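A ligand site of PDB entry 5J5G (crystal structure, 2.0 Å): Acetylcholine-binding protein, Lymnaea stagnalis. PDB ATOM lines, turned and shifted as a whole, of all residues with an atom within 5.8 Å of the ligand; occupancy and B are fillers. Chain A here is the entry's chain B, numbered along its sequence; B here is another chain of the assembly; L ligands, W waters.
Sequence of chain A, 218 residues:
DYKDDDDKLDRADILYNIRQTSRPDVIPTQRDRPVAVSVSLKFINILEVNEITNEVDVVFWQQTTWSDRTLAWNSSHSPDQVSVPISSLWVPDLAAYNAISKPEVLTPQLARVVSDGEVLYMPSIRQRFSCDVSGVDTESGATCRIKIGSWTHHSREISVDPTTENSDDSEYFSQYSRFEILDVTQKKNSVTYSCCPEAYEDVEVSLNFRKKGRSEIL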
ATOM      1  N   SER A  38     -23.360   5.969   5.535  1.00  0.00           N
ATOM      2  CA  SER A  38     -24.305   5.897   4.425  1.00  0.00           C
ATOM      3  C   SER A  38     -23.816   6.774   3.271  1.00  0.00           C
ATOM      4  O   SER A  38     -23.424   7.922   3.473  1.00  0.00           O
ATOM      5  CB  SER A  38     -25.704   6.341   4.857  1.00  0.00           C
ATOM      6  OG  SER A  38     -26.118   5.584   5.971  1.00  0.00           O
ATOM      7  N   VAL A  39     -23.837   6.200   2.070  1.00  0.00           N
ATOM      8  CA  VAL A  39     -23.278   6.799   0.873  1.00  0.00           C
ATOM      9  C   VAL A  39     -24.269   6.721  -0.257  1.00  0.00           C
ATOM     10  O   VAL A  39     -24.861   5.679  -0.520  1.00  0.00           O
ATOM     11  CB  VAL A  39     -21.976   6.092   0.423  1.00  0.00           C
ATOM     12  CG1 VAL A  39     -21.390   6.790  -0.804  1.00  0.00           C
ATOM     13  CG2 VAL A  39     -20.969   6.055   1.533  1.00  0.00           C
ATOM     14  N   SER A  40     -24.451   7.835  -0.962  1.00  0.00           N
ATOM     15  CA  SER A  40     -25.282   7.834  -2.145  1.00  0.00           C
ATOM     16  C   SER A  40     -24.700   8.802  -3.173  1.00  0.00           C
ATOM     17  O   SER A  40     -24.647  10.004  -2.926  1.00  0.00           O
ATOM     18  CB  SER A  40     -26.721   8.218  -1.799  1.00  0.00           C
ATOM     19  OG  SER A  40     -27.512   8.289  -2.967  1.00  0.00           O
ATOM     20  N   TRP A  61     -21.944  14.191  -6.869  1.00  0.00           N
ATOM     21  CA  TRP A  61     -21.964  14.618  -5.477  1.00  0.00           C
ATOM     22  C   TRP A  61     -22.016  13.367  -4.642  1.00  0.00           C
ATOM     23  O   TRP A  61     -22.935  12.554  -4.790  1.00  0.00           O
ATOM     24  CB  TRP A  61     -23.176  15.526  -5.180  1.00  0.00           C
ATOM     25  CG  TRP A  61     -23.165  16.824  -5.947  1.00  0.00           C
ATOM     26  CD1 TRP A  61     -22.201  17.275  -6.806  1.00  0.00           C
ATOM     27  CD2 TRP A  61     -24.173  17.843  -5.918  1.00  0.00           C
ATOM     28  NE1 TRP A  61     -22.545  18.507  -7.305  1.00  0.00           N
ATOM     29  CE2 TRP A  61     -23.745  18.877  -6.779  1.00  0.00           C
ATOM     30  CE3 TRP A  61     -25.391  17.971  -5.244  1.00  0.00           C
ATOM     31  CZ2 TRP A  61     -24.499  20.032  -6.987  1.00  0.00           C
ATOM     32  CZ3 TRP A  61     -26.140  19.130  -5.459  1.00  0.00           C
ATOM     33  CH2 TRP A  61     -25.690  20.143  -6.319  1.00  0.00           C
ATOM     34  N   GLN A  62     -21.013  13.179  -3.795  1.00  0.00           N
ATOM     35  CA  GLN A  62     -20.945  12.014  -2.927  1.00  0.00           C
ATOM     36  C   GLN A  62     -21.664  12.298  -1.608  1.00  0.00           C
ATOM     37  O   GLN A  62     -21.042  12.790  -0.661  1.00  0.00           O
ATOM     38  CB  GLN A  62     -19.495  11.619  -2.689  1.00  0.00           C
ATOM     39  CG  GLN A  62     -19.303  10.427  -1.772  1.00  0.00           C
ATOM     40  CD  GLN A  62     -17.842  10.288  -1.336  1.00  0.00           C
ATOM     41  OE1 GLN A  62     -16.975   9.973  -2.144  1.00  0.00           O
ATOM     42  NE2 GLN A  62     -17.570  10.579  -0.067  1.00  0.00           N
ATOM     43  N   GLN A  63     -22.958  12.003  -1.550  1.00  0.00           N
ATOM     44  CA  GLN A  63     -23.745  12.224  -0.339  1.00  0.00           C
ATOM     45  C   GLN A  63     -23.301  11.217   0.715  1.00  0.00           C
ATOM     46  O   GLN A  63     -23.426  10.001   0.520  1.00  0.00           O
ATOM     47  CB  GLN A  63     -25.251  12.107  -0.625  1.00  0.00           C
ATOM     48  CG  GLN A  63     -25.781  13.144  -1.608  1.00  0.00           C
ATOM     49  CD  GLN A  63     -27.281  13.035  -1.859  1.00  0.00           C
ATOM     50  OE1 GLN A  63     -28.008  14.028  -1.856  1.00  0.00           O
ATOM     51  NE2 GLN A  63     -27.757  11.799  -2.074  1.00  0.00           N
ATOM     52  N   THR A  64     -22.732  11.707   1.812  1.00  0.00           N
ATOM     53  CA  THR A  64     -22.153  10.853   2.829  1.00  0.00           C
ATOM     54  C   THR A  64     -22.654  11.268   4.203  1.00  0.00           C
ATOM     55  O   THR A  64     -22.684  12.458   4.510  1.00  0.00           O
ATOM     56  CB  THR A  64     -20.610  10.904   2.821  1.00  0.00           C
ATOM     57  OG1 THR A  64     -20.145  11.076   1.471  1.00  0.00           O
ATOM     58  CG2 THR A  64     -20.005   9.647   3.417  1.00  0.00           C
ATOM     59  N   THR A  65     -23.056  10.302   5.015  1.00  0.00           N
ATOM     60  CA  THR A  65     -23.463  10.626   6.380  1.00  0.00           C
ATOM     61  C   THR A  65     -23.121   9.492   7.347  1.00  0.00           C
ATOM     62  O   THR A  65     -23.004   8.329   6.965  1.00  0.00           O
ATOM     63  CB  THR A  65     -24.979  10.969   6.454  1.00  0.00           C
ATOM     64  OG1 THR A  65     -25.260  11.565   7.730  1.00  0.00           O
ATOM     65  CG2 THR A  65     -25.852   9.725   6.291  1.00  0.00           C
ATOM     66  N   LEU A 110     -16.128  21.407   3.621  1.00  0.00           N
ATOM     67  CA  LEU A 110     -16.854  21.592   4.863  1.00  0.00           C
ATOM     68  C   LEU A 110     -17.899  20.507   5.017  1.00  0.00           C
ATOM     69  O   LEU A 110     -18.439  20.011   4.040  1.00  0.00           O
ATOM     70  CB  LEU A 110     -17.546  22.956   4.885  1.00  0.00           C
ATOM     71  CG  LEU A 110     -16.712  24.211   4.700  1.00  0.00           C
ATOM     72  CD1 LEU A 110     -17.655  25.391   4.601  1.00  0.00           C
ATOM     73  CD2 LEU A 110     -15.749  24.379   5.880  1.00  0.00           C
ATOM     74  N   ALA A 111     -18.183  20.140   6.259  1.00  0.00           N
ATOM     75  CA  ALA A 111     -19.281  19.238   6.541  1.00  0.00           C
ATOM     76  C   ALA A 111     -20.277  19.959   7.417  1.00  0.00           C
ATOM     77  O   ALA A 111     -19.990  21.046   7.953  1.00  0.00           O
ATOM     78  CB  ALA A 111     -18.789  17.939   7.213  1.00  0.00           C
ATOM     79  N   ARG A 112     -21.462  19.392   7.566  1.00  0.00           N
ATOM     80  CA  ARG A 112     -22.434  19.912   8.523  1.00  0.00           C
ATOM     81  C   ARG A 112     -22.449  18.997   9.713  1.00  0.00           C
ATOM     82  O   ARG A 112     -22.516  17.785   9.544  1.00  0.00           O
ATOM     83  CB  ARG A 112     -23.837  19.998   7.920  1.00  0.00           C
ATOM     84  CG  ARG A 112     -23.960  21.005   6.803  1.00  0.00           C
ATOM     85  CD  ARG A 112     -23.920  22.429   7.359  1.00  0.00           C
ATOM     86  NE  ARG A 112     -25.179  22.872   7.958  1.00  0.00           N
ATOM     87  CZ  ARG A 112     -25.401  24.126   8.327  1.00  0.00           C
ATOM     88  NH1 ARG A 112     -24.446  25.031   8.169  1.00  0.00           N
ATOM     89  NH2 ARG A 112     -26.579  24.504   8.845  1.00  0.00           N
ATOM     90  N   GLU A 118     -25.167  13.718  14.079  1.00  0.00           N
ATOM     91  CA  GLU A 118     -25.065  13.347  12.667  1.00  0.00           C
ATOM     92  C   GLU A 118     -24.127  14.300  11.945  1.00  0.00           C
ATOM     93  O   GLU A 118     -24.125  15.521  12.185  1.00  0.00           O
ATOM     94  CB  GLU A 118     -26.447  13.336  11.980  1.00  0.00           C
ATOM     95  CG  GLU A 118     -26.416  12.646  10.610  1.00  0.00           C
ATOM     96  CD  GLU A 118     -27.695  12.807   9.799  1.00  0.00           C
ATOM     97  OE1 GLU A 118     -28.643  13.454  10.305  1.00  0.00           O
ATOM     98  OE2 GLU A 118     -27.748  12.291   8.665  1.00  0.00           O
ATOM     99  N   LEU A 120     -22.953  15.437   8.044  1.00  0.00           N
ATOM    100  CA  LEU A 120     -23.247  15.375   6.608  1.00  0.00           C
ATOM    101  C   LEU A 120     -22.088  15.960   5.805  1.00  0.00           C
ATOM    102  O   LEU A 120     -21.681  17.097   6.036  1.00  0.00           O
ATOM    103  CB  LEU A 120     -24.538  16.118   6.268  1.00  0.00           C
ATOM    104  CG  LEU A 120     -25.815  15.602   6.918  1.00  0.00           C
ATOM    105  CD1 LEU A 120     -26.163  16.496   8.065  1.00  0.00           C
ATOM    106  CD2 LEU A 120     -26.963  15.571   5.930  1.00  0.00           C
ATOM    107  N   TYR A 121     -21.592  15.190   4.850  1.00  0.00           N
ATOM    108  CA  TYR A 121     -20.492  15.610   4.005  1.00  0.00           C
ATOM    109  C   TYR A 121     -20.814  15.270   2.557  1.00  0.00           C
ATOM    110  O   TYR A 121     -21.196  14.140   2.240  1.00  0.00           O
ATOM    111  CB  TYR A 121     -19.201  14.917   4.455  1.00  0.00           C
ATOM    112  CG  TYR A 121     -17.986  15.137   3.589  1.00  0.00           C
ATOM    113  CD1 TYR A 121     -17.508  16.418   3.303  1.00  0.00           C
ATOM    114  CD2 TYR A 121     -17.262  14.039   3.111  1.00  0.00           C
ATOM    115  CE1 TYR A 121     -16.357  16.591   2.527  1.00  0.00           C
ATOM    116  CE2 TYR A 121     -16.121  14.202   2.336  1.00  0.00           C
ATOM    117  CZ  TYR A 121     -15.675  15.465   2.059  1.00  0.00           C
ATOM    118  OH  TYR A 121     -14.561  15.584   1.282  1.00  0.00           O
ATOM    119  N   MET A 122     -20.686  16.234   1.651  1.00  0.00           N
ATOM    120  CA  MET A 122     -21.091  16.000   0.267  1.00  0.00           C
ATOM    121  C   MET A 122     -20.177  16.756  -0.666  1.00  0.00           C
ATOM    122  O   MET A 122     -20.500  17.853  -1.140  1.00  0.00           O
ATOM    123  CB  MET A 122     -22.565  16.399   0.044  1.00  0.00           C
ATOM    124  CG  MET A 122     -23.123  16.004  -1.360  1.00  0.00           C
ATOM    125  SD  MET A 122     -24.805  16.614  -1.667  1.00  0.00           S
ATOM    126  CE  MET A 122     -24.497  18.378  -1.811  1.00  0.00           C
ATOM    127  N   THR A 163     -28.080   4.518   0.578  1.00  0.00           N
ATOM    128  CA  THR A 163     -29.267   5.163   1.131  1.00  0.00           C
ATOM    129  C   THR A 163     -30.515   4.750   0.368  1.00  0.00           C
ATOM    130  O   THR A 163     -31.419   4.141   0.919  1.00  0.00           O
ATOM    131  CB  THR A 163     -29.141   6.700   1.094  1.00  0.00           C
ATOM    132  OG1 THR A 163     -27.835   7.095   1.553  1.00  0.00           O
ATOM    133  CG2 THR A 163     -30.215   7.338   1.965  1.00  0.00           C
ATOM    134  N   TYR A 172     -30.464  16.171 -10.300  1.00  0.00           N
ATOM    135  CA  TYR A 172     -29.034  16.457 -10.225  1.00  0.00           C
ATOM    136  C   TYR A 172     -28.331  16.431 -11.571  1.00  0.00           C
ATOM    137  O   TYR A 172     -27.437  17.235 -11.841  1.00  0.00           O
ATOM    138  CB  TYR A 172     -28.342  15.457  -9.276  1.00  0.00           C
ATOM    139  CG  TYR A 172     -28.847  15.510  -7.830  1.00  0.00           C
ATOM    140  CD1 TYR A 172     -28.171  16.248  -6.861  1.00  0.00           C
ATOM    141  CD2 TYR A 172     -29.985  14.804  -7.443  1.00  0.00           C
ATOM    142  CE1 TYR A 172     -28.640  16.301  -5.550  1.00  0.00           C
ATOM    143  CE2 TYR A 172     -30.451  14.845  -6.138  1.00  0.00           C
ATOM    144  CZ  TYR A 172     -29.779  15.593  -5.192  1.00  0.00           C
ATOM    145  OH  TYR A 172     -30.245  15.633  -3.901  1.00  0.00           O
ATOM    146  N   TYR B  97     -22.500  25.361  -8.866  1.00  0.00           N
ATOM    147  CA  TYR B  97     -23.186  24.079  -8.817  1.00  0.00           C
ATOM    148  C   TYR B  97     -22.988  23.266 -10.102  1.00  0.00           C
ATOM    149  O   TYR B  97     -23.110  22.037 -10.091  1.00  0.00           O
ATOM    150  CB  TYR B  97     -24.683  24.298  -8.514  1.00  0.00           C
ATOM    151  CG  TYR B  97     -24.976  24.944  -7.163  1.00  0.00           C
ATOM    152  CD1 TYR B  97     -23.960  25.223  -6.242  1.00  0.00           C
ATOM    153  CD2 TYR B  97     -26.283  25.264  -6.787  1.00  0.00           C
ATOM    154  CE1 TYR B  97     -24.234  25.810  -4.993  1.00  0.00           C
ATOM    155  CE2 TYR B  97     -26.566  25.841  -5.537  1.00  0.00           C
ATOM    156  CZ  TYR B  97     -25.542  26.129  -4.645  1.00  0.00           C
ATOM    157  OH  TYR B  97     -25.845  26.714  -3.402  1.00  0.00           O
ATOM    158  N   SER B 150     -23.742  29.283  -1.692  1.00  0.00           N
ATOM    159  CA  SER B 150     -23.056  28.619  -0.601  1.00  0.00           C
ATOM    160  C   SER B 150     -23.151  27.106  -0.715  1.00  0.00           C
ATOM    161  O   SER B 150     -24.221  26.562  -0.982  1.00  0.00           O
ATOM    162  CB  SER B 150     -23.633  29.054   0.752  1.00  0.00           C
ATOM    163  OG  SER B 150     -23.048  28.295   1.789  1.00  0.00           O
ATOM    164  N   TRP B 151     -22.036  26.404  -0.474  1.00  0.00           N
ATOM    165  CA  TRP B 151     -22.069  24.945  -0.531  1.00  0.00           C
ATOM    166  C   TRP B 151     -22.747  24.295   0.680  1.00  0.00           C
ATOM    167  O   TRP B 151     -23.333  23.222   0.546  1.00  0.00           O
ATOM    168  CB  TRP B 151     -20.635  24.381  -0.669  1.00  0.00           C
ATOM    169  CG  TRP B 151     -20.657  22.929  -1.031  1.00  0.00           C
ATOM    170  CD1 TRP B 151     -20.108  21.895  -0.326  1.00  0.00           C
ATOM    171  CD2 TRP B 151     -21.257  22.345  -2.192  1.00  0.00           C
ATOM    172  NE1 TRP B 151     -20.337  20.701  -0.982  1.00  0.00           N
ATOM    173  CE2 TRP B 151     -21.040  20.953  -2.131  1.00  0.00           C
ATOM    174  CE3 TRP B 151     -21.964  22.872  -3.285  1.00  0.00           C
ATOM    175  CZ2 TRP B 151     -21.501  20.076  -3.113  1.00  0.00           C
ATOM    176  CZ3 TRP B 151     -22.425  21.995  -4.268  1.00  0.00           C
ATOM    177  CH2 TRP B 151     -22.192  20.621  -4.173  1.00  0.00           C
ATOM    178  N   THR B 152     -22.645  24.908   1.862  1.00  0.00           N
ATOM    179  CA  THR B 152     -23.165  24.264   3.082  1.00  0.00           C
ATOM    180  C   THR B 152     -24.119  25.128   3.925  1.00  0.00           C
ATOM    181  O   THR B 152     -24.661  24.650   4.926  1.00  0.00           O
ATOM    182  CB  THR B 152     -22.008  23.810   4.026  1.00  0.00           C
ATOM    183  OG1 THR B 152     -21.356  24.963   4.606  1.00  0.00           O
ATOM    184  CG2 THR B 152     -20.991  22.972   3.265  1.00  0.00           C
ATOM    185  N   VAL B 191     -32.636  27.191  -4.623  1.00  0.00           N
ATOM    186  CA  VAL B 191     -32.486  25.780  -4.907  1.00  0.00           C
ATOM    187  C   VAL B 191     -32.922  24.947  -3.693  1.00  0.00           C
ATOM    188  O   VAL B 191     -32.565  25.261  -2.556  1.00  0.00           O
ATOM    189  CB  VAL B 191     -31.038  25.432  -5.291  1.00  0.00           C
ATOM    190  CG1 VAL B 191     -30.827  23.942  -5.293  1.00  0.00           C
ATOM    191  CG2 VAL B 191     -30.684  26.023  -6.660  1.00  0.00           C
ATOM    192  N   TYR B 193     -33.874  20.533  -2.649  1.00  0.00           N
ATOM    193  CA  TYR B 193     -33.873  19.131  -3.073  1.00  0.00           C
ATOM    194  C   TYR B 193     -34.889  18.332  -2.269  1.00  0.00           C
ATOM    195  O   TYR B 193     -35.206  18.692  -1.143  1.00  0.00           O
ATOM    196  CB  TYR B 193     -32.463  18.531  -2.917  1.00  0.00           C
ATOM    197  CG  TYR B 193     -31.475  19.220  -3.817  1.00  0.00           C
ATOM    198  CD1 TYR B 193     -31.376  18.880  -5.161  1.00  0.00           C
ATOM    199  CD2 TYR B 193     -30.676  20.262  -3.331  1.00  0.00           C
ATOM    200  CE1 TYR B 193     -30.497  19.532  -6.006  1.00  0.00           C
ATOM    201  CE2 TYR B 193     -29.773  20.911  -4.177  1.00  0.00           C
ATOM    202  CZ  TYR B 193     -29.698  20.545  -5.510  1.00  0.00           C
ATOM    203  OH  TYR B 193     -28.821  21.180  -6.354  1.00  0.00           O
ATOM    204  N   CYS B 195     -34.563  15.475  -1.003  1.00  0.00           N
ATOM    205  CA  CYS B 195     -33.904  14.798   0.104  1.00  0.00           C
ATOM    206  C   CYS B 195     -33.862  15.672   1.350  1.00  0.00           C
ATOM    207  O   CYS B 195     -33.868  15.183   2.470  1.00  0.00           O
ATOM    208  CB  CYS B 195     -32.478  14.413  -0.277  1.00  0.00           C
ATOM    209  SG  CYS B 195     -31.382  15.864  -0.299  1.00  0.00           S
ATOM    210  N   CYS B 196     -33.812  16.987   1.134  1.00  0.00           N
ATOM    211  CA  CYS B 196     -33.361  17.872   2.194  1.00  0.00           C
ATOM    212  C   CYS B 196     -34.303  19.045   2.422  1.00  0.00           C
ATOM    213  O   CYS B 196     -34.948  19.531   1.501  1.00  0.00           O
ATOM    214  CB  CYS B 196     -31.937  18.359   1.870  1.00  0.00           C
ATOM    215  SG  CYS B 196     -30.856  17.009   1.320  1.00  0.00           S
ATOM    216  N   TYR B 200     -31.481  26.881  -0.569  1.00  0.00           N
ATOM    217  CA  TYR B 200     -30.185  27.519  -0.712  1.00  0.00           C
ATOM    218  C   TYR B 200     -30.289  28.624  -1.745  1.00  0.00           C
ATOM    219  O   TYR B 200     -30.750  28.390  -2.873  1.00  0.00           O
ATOM    220  CB  TYR B 200     -29.119  26.497  -1.089  1.00  0.00           C
ATOM    221  CG  TYR B 200     -28.730  25.612   0.069  1.00  0.00           C
ATOM    222  CD1 TYR B 200     -29.655  24.752   0.656  1.00  0.00           C
ATOM    223  CD2 TYR B 200     -27.451  25.637   0.594  1.00  0.00           C
ATOM    224  CE1 TYR B 200     -29.327  23.958   1.737  1.00  0.00           C
ATOM    225  CE2 TYR B 200     -27.109  24.829   1.676  1.00  0.00           C
ATOM    226  CZ  TYR B 200     -28.045  23.998   2.246  1.00  0.00           C
ATOM    227  OH  TYR B 200     -27.711  23.197   3.313  1.00  0.00           O
HETATM  228  C1  LIG L   1     -27.315  18.772   0.768  1.00  0.00           C
HETATM  229  C2  LIG L   1     -25.072  19.957   2.562  1.00  0.00           C
HETATM  230  C3  LIG L   1     -23.064  19.110   3.606  1.00  0.00           C
HETATM  231  C4  LIG L   1     -22.970  20.134   1.433  1.00  0.00           C
HETATM  232  C5  LIG L   1     -24.961  21.936  -1.834  1.00  0.00           C
HETATM  233  C6  LIG L   1     -25.650  22.678  -2.789  1.00  0.00           C
HETATM  234  C7  LIG L   1     -27.008  22.919  -2.597  1.00  0.00           C
HETATM  235  C8  LIG L   1     -26.395  10.325   2.633  1.00  0.00           C
HETATM  236  O1  LIG L   1     -25.945  11.531   3.276  1.00  0.00           O
HETATM  237  C9  LIG L   1     -26.306  12.711   2.682  1.00  0.00           C
HETATM  238  C10 LIG L   1     -25.481  13.832   2.835  1.00  0.00           C
HETATM  239  C11 LIG L   1     -25.820  15.050   2.238  1.00  0.00           C
HETATM  240  C12 LIG L   1     -27.475  12.832   1.930  1.00  0.00           C
HETATM  241  C13 LIG L   1     -27.802  14.048   1.325  1.00  0.00           C
HETATM  242  C14 LIG L   1     -26.981  15.164   1.486  1.00  0.00           C
HETATM  243  C15 LIG L   1     -27.304  16.384   0.873  1.00  0.00           C
HETATM  244  C16 LIG L   1     -26.976  17.604   1.461  1.00  0.00           C
HETATM  245  N1  LIG L   1     -27.910  16.370  -0.334  1.00  0.00           N
HETATM  246  C17 LIG L   1     -28.233  17.501  -0.960  1.00  0.00           C
HETATM  247  N2  LIG L   1     -28.847  17.466  -2.158  1.00  0.00           N
HETATM  248  N3  LIG L   1     -27.931  18.692  -0.419  1.00  0.00           N
HETATM  249  N4  LIG L   1     -27.067  19.992   1.280  1.00  0.00           N
HETATM  250  C18 LIG L   1     -27.608  21.212   0.637  1.00  0.00           C
HETATM  251  C19 LIG L   1     -26.933  21.676  -0.501  1.00  0.00           C
HETATM  252  N5  LIG L   1     -25.626  21.454  -0.687  1.00  0.00           N
HETATM  253  C20 LIG L   1     -27.634  22.420  -1.450  1.00  0.00           C
HETATM  254  C21 LIG L   1     -26.445  20.189   2.606  1.00  0.00           C
HETATM  255  N6  LIG L   1     -24.357  20.350   1.486  1.00  0.00           N
HETATM  256  C22 LIG L   1     -22.328  19.508   2.493  1.00  0.00           C
HETATM  257  C23 LIG L   1     -24.437  19.340   3.636  1.00  0.00           C
HETATM  258  O   HOH W   1     -27.295  20.445   5.967  1.00  0.00           O
HETATM  259  O   HOH W   2     -19.205  18.835   1.498  1.00  0.00           O
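OE1 of Gln 63 sits close to N1 of the ligand (2.8 Å). N2 of the ligand lies within hydrogen-bond range of OH of Tyr 172, at 2.9 Å. The side-chain sulfur (SG) of Cys 195 of chain B is in hydrogen-bond range of a nitrogen (N2) of the ligand, 3.5 Å away.
OE1 of Gln 63 is in hydrogen-bond range of OH of Tyr 172 (3.4 Å). The backbone carbonyl oxygen (O) of Gln 63 sits at hydrogen-bond distance from the backbone NH (N) of Ser 40 (2.8 Å). The side-chain hydroxyl (OH) of Tyr 172 is in hydrogen-bond range of the side-chain sulfur (SG) of Cys 195 of chain B (3.8 Å). The backbone NH (N) of Tyr 200 of chain B lies within hydrogen-bond range of the backbone carbonyl oxygen (O) of Val 191 of chain B, at 2.8 Å. The side-chain carboxylate of Glu 118 lies within hydrogen-bond range of the side-chain hydroxyl of Thr 65, at 2.8 Å. The backbone NH of Thr 64 sits at hydrogen-bond distance from the backbone carbonyl oxygen of Tyr 121, 2.9 Å away. SG of Cys 195 of chain B forms a disulfide with SG of Cys 196 of chain B, at 2.1 Å. The backbone NH (N) of Thr 152 of chain B lies within hydrogen-bond range of the side-chain hydroxyl (OG) of Ser 150 of chain B, 3.4 Å away.
The side-chain sulfur (SD) of Met 122 lies close to a nitrogen (N1) of the ligand, 3.4 Å away. The backbone carbonyl oxygen (O) of Trp 151 of chain B sits close to a nitrogen (N5) of the ligand, 3.1 Å away. The side-chain sulfur (SG) of Cys 196 of chain B sits close to a nitrogen (N1) of the ligand. O of Ser 38 touches C8 of the ligand, at 3.9 Å. C of Thr 64 touches O1 of the ligand, 3.4 Å away. Thr 65 touches the ligand. Arg 112 touches the ligand. Leu 120 touches the ligand. Thr 163 touches the ligand. Tyr 97 of chain B touches the ligand (CZ to C6, 3.9 Å). Thr 152 of chain B touches the ligand (CG2 to C22, 3.8 Å). Tyr 193 of chain B touches the ligand. CZ of Tyr 200 of chain B touches C18 of the ligand, 3.2 Å away. Hydrophobic or aromatic side chains within 4 Å of the ligand: Leu 120, Met 122, Tyr 172, Tyr 97 of chain B, Trp 151 of chain B, Tyr 193 of chain B and Tyr 200 of chain B. 16 residues have an atom within 4 Å of the ligand: Ser 38, Gln 63, Thr 64, Thr 65, Arg 112, Leu 120, Met 122, Thr 163, Tyr 172, Tyr 97 of chain B, Trp 151 of chain B, Thr 152 of chain B, Tyr 193 of chain B, Cys 195 of chain B, Cys 196 of chain B and Tyr 200 of chain B. The nearest printed residue that does not touch the ligand is Leu 110 (4.2 Å).
Water W2 lies within hydrogen-bond range of the backbone carbonyl oxygen of Leu 110 (2.9 Å), the backbone NH of Met 122 (3.0 Å) and the indole nitrogen of Trp 151 of chain B (3.3 Å).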
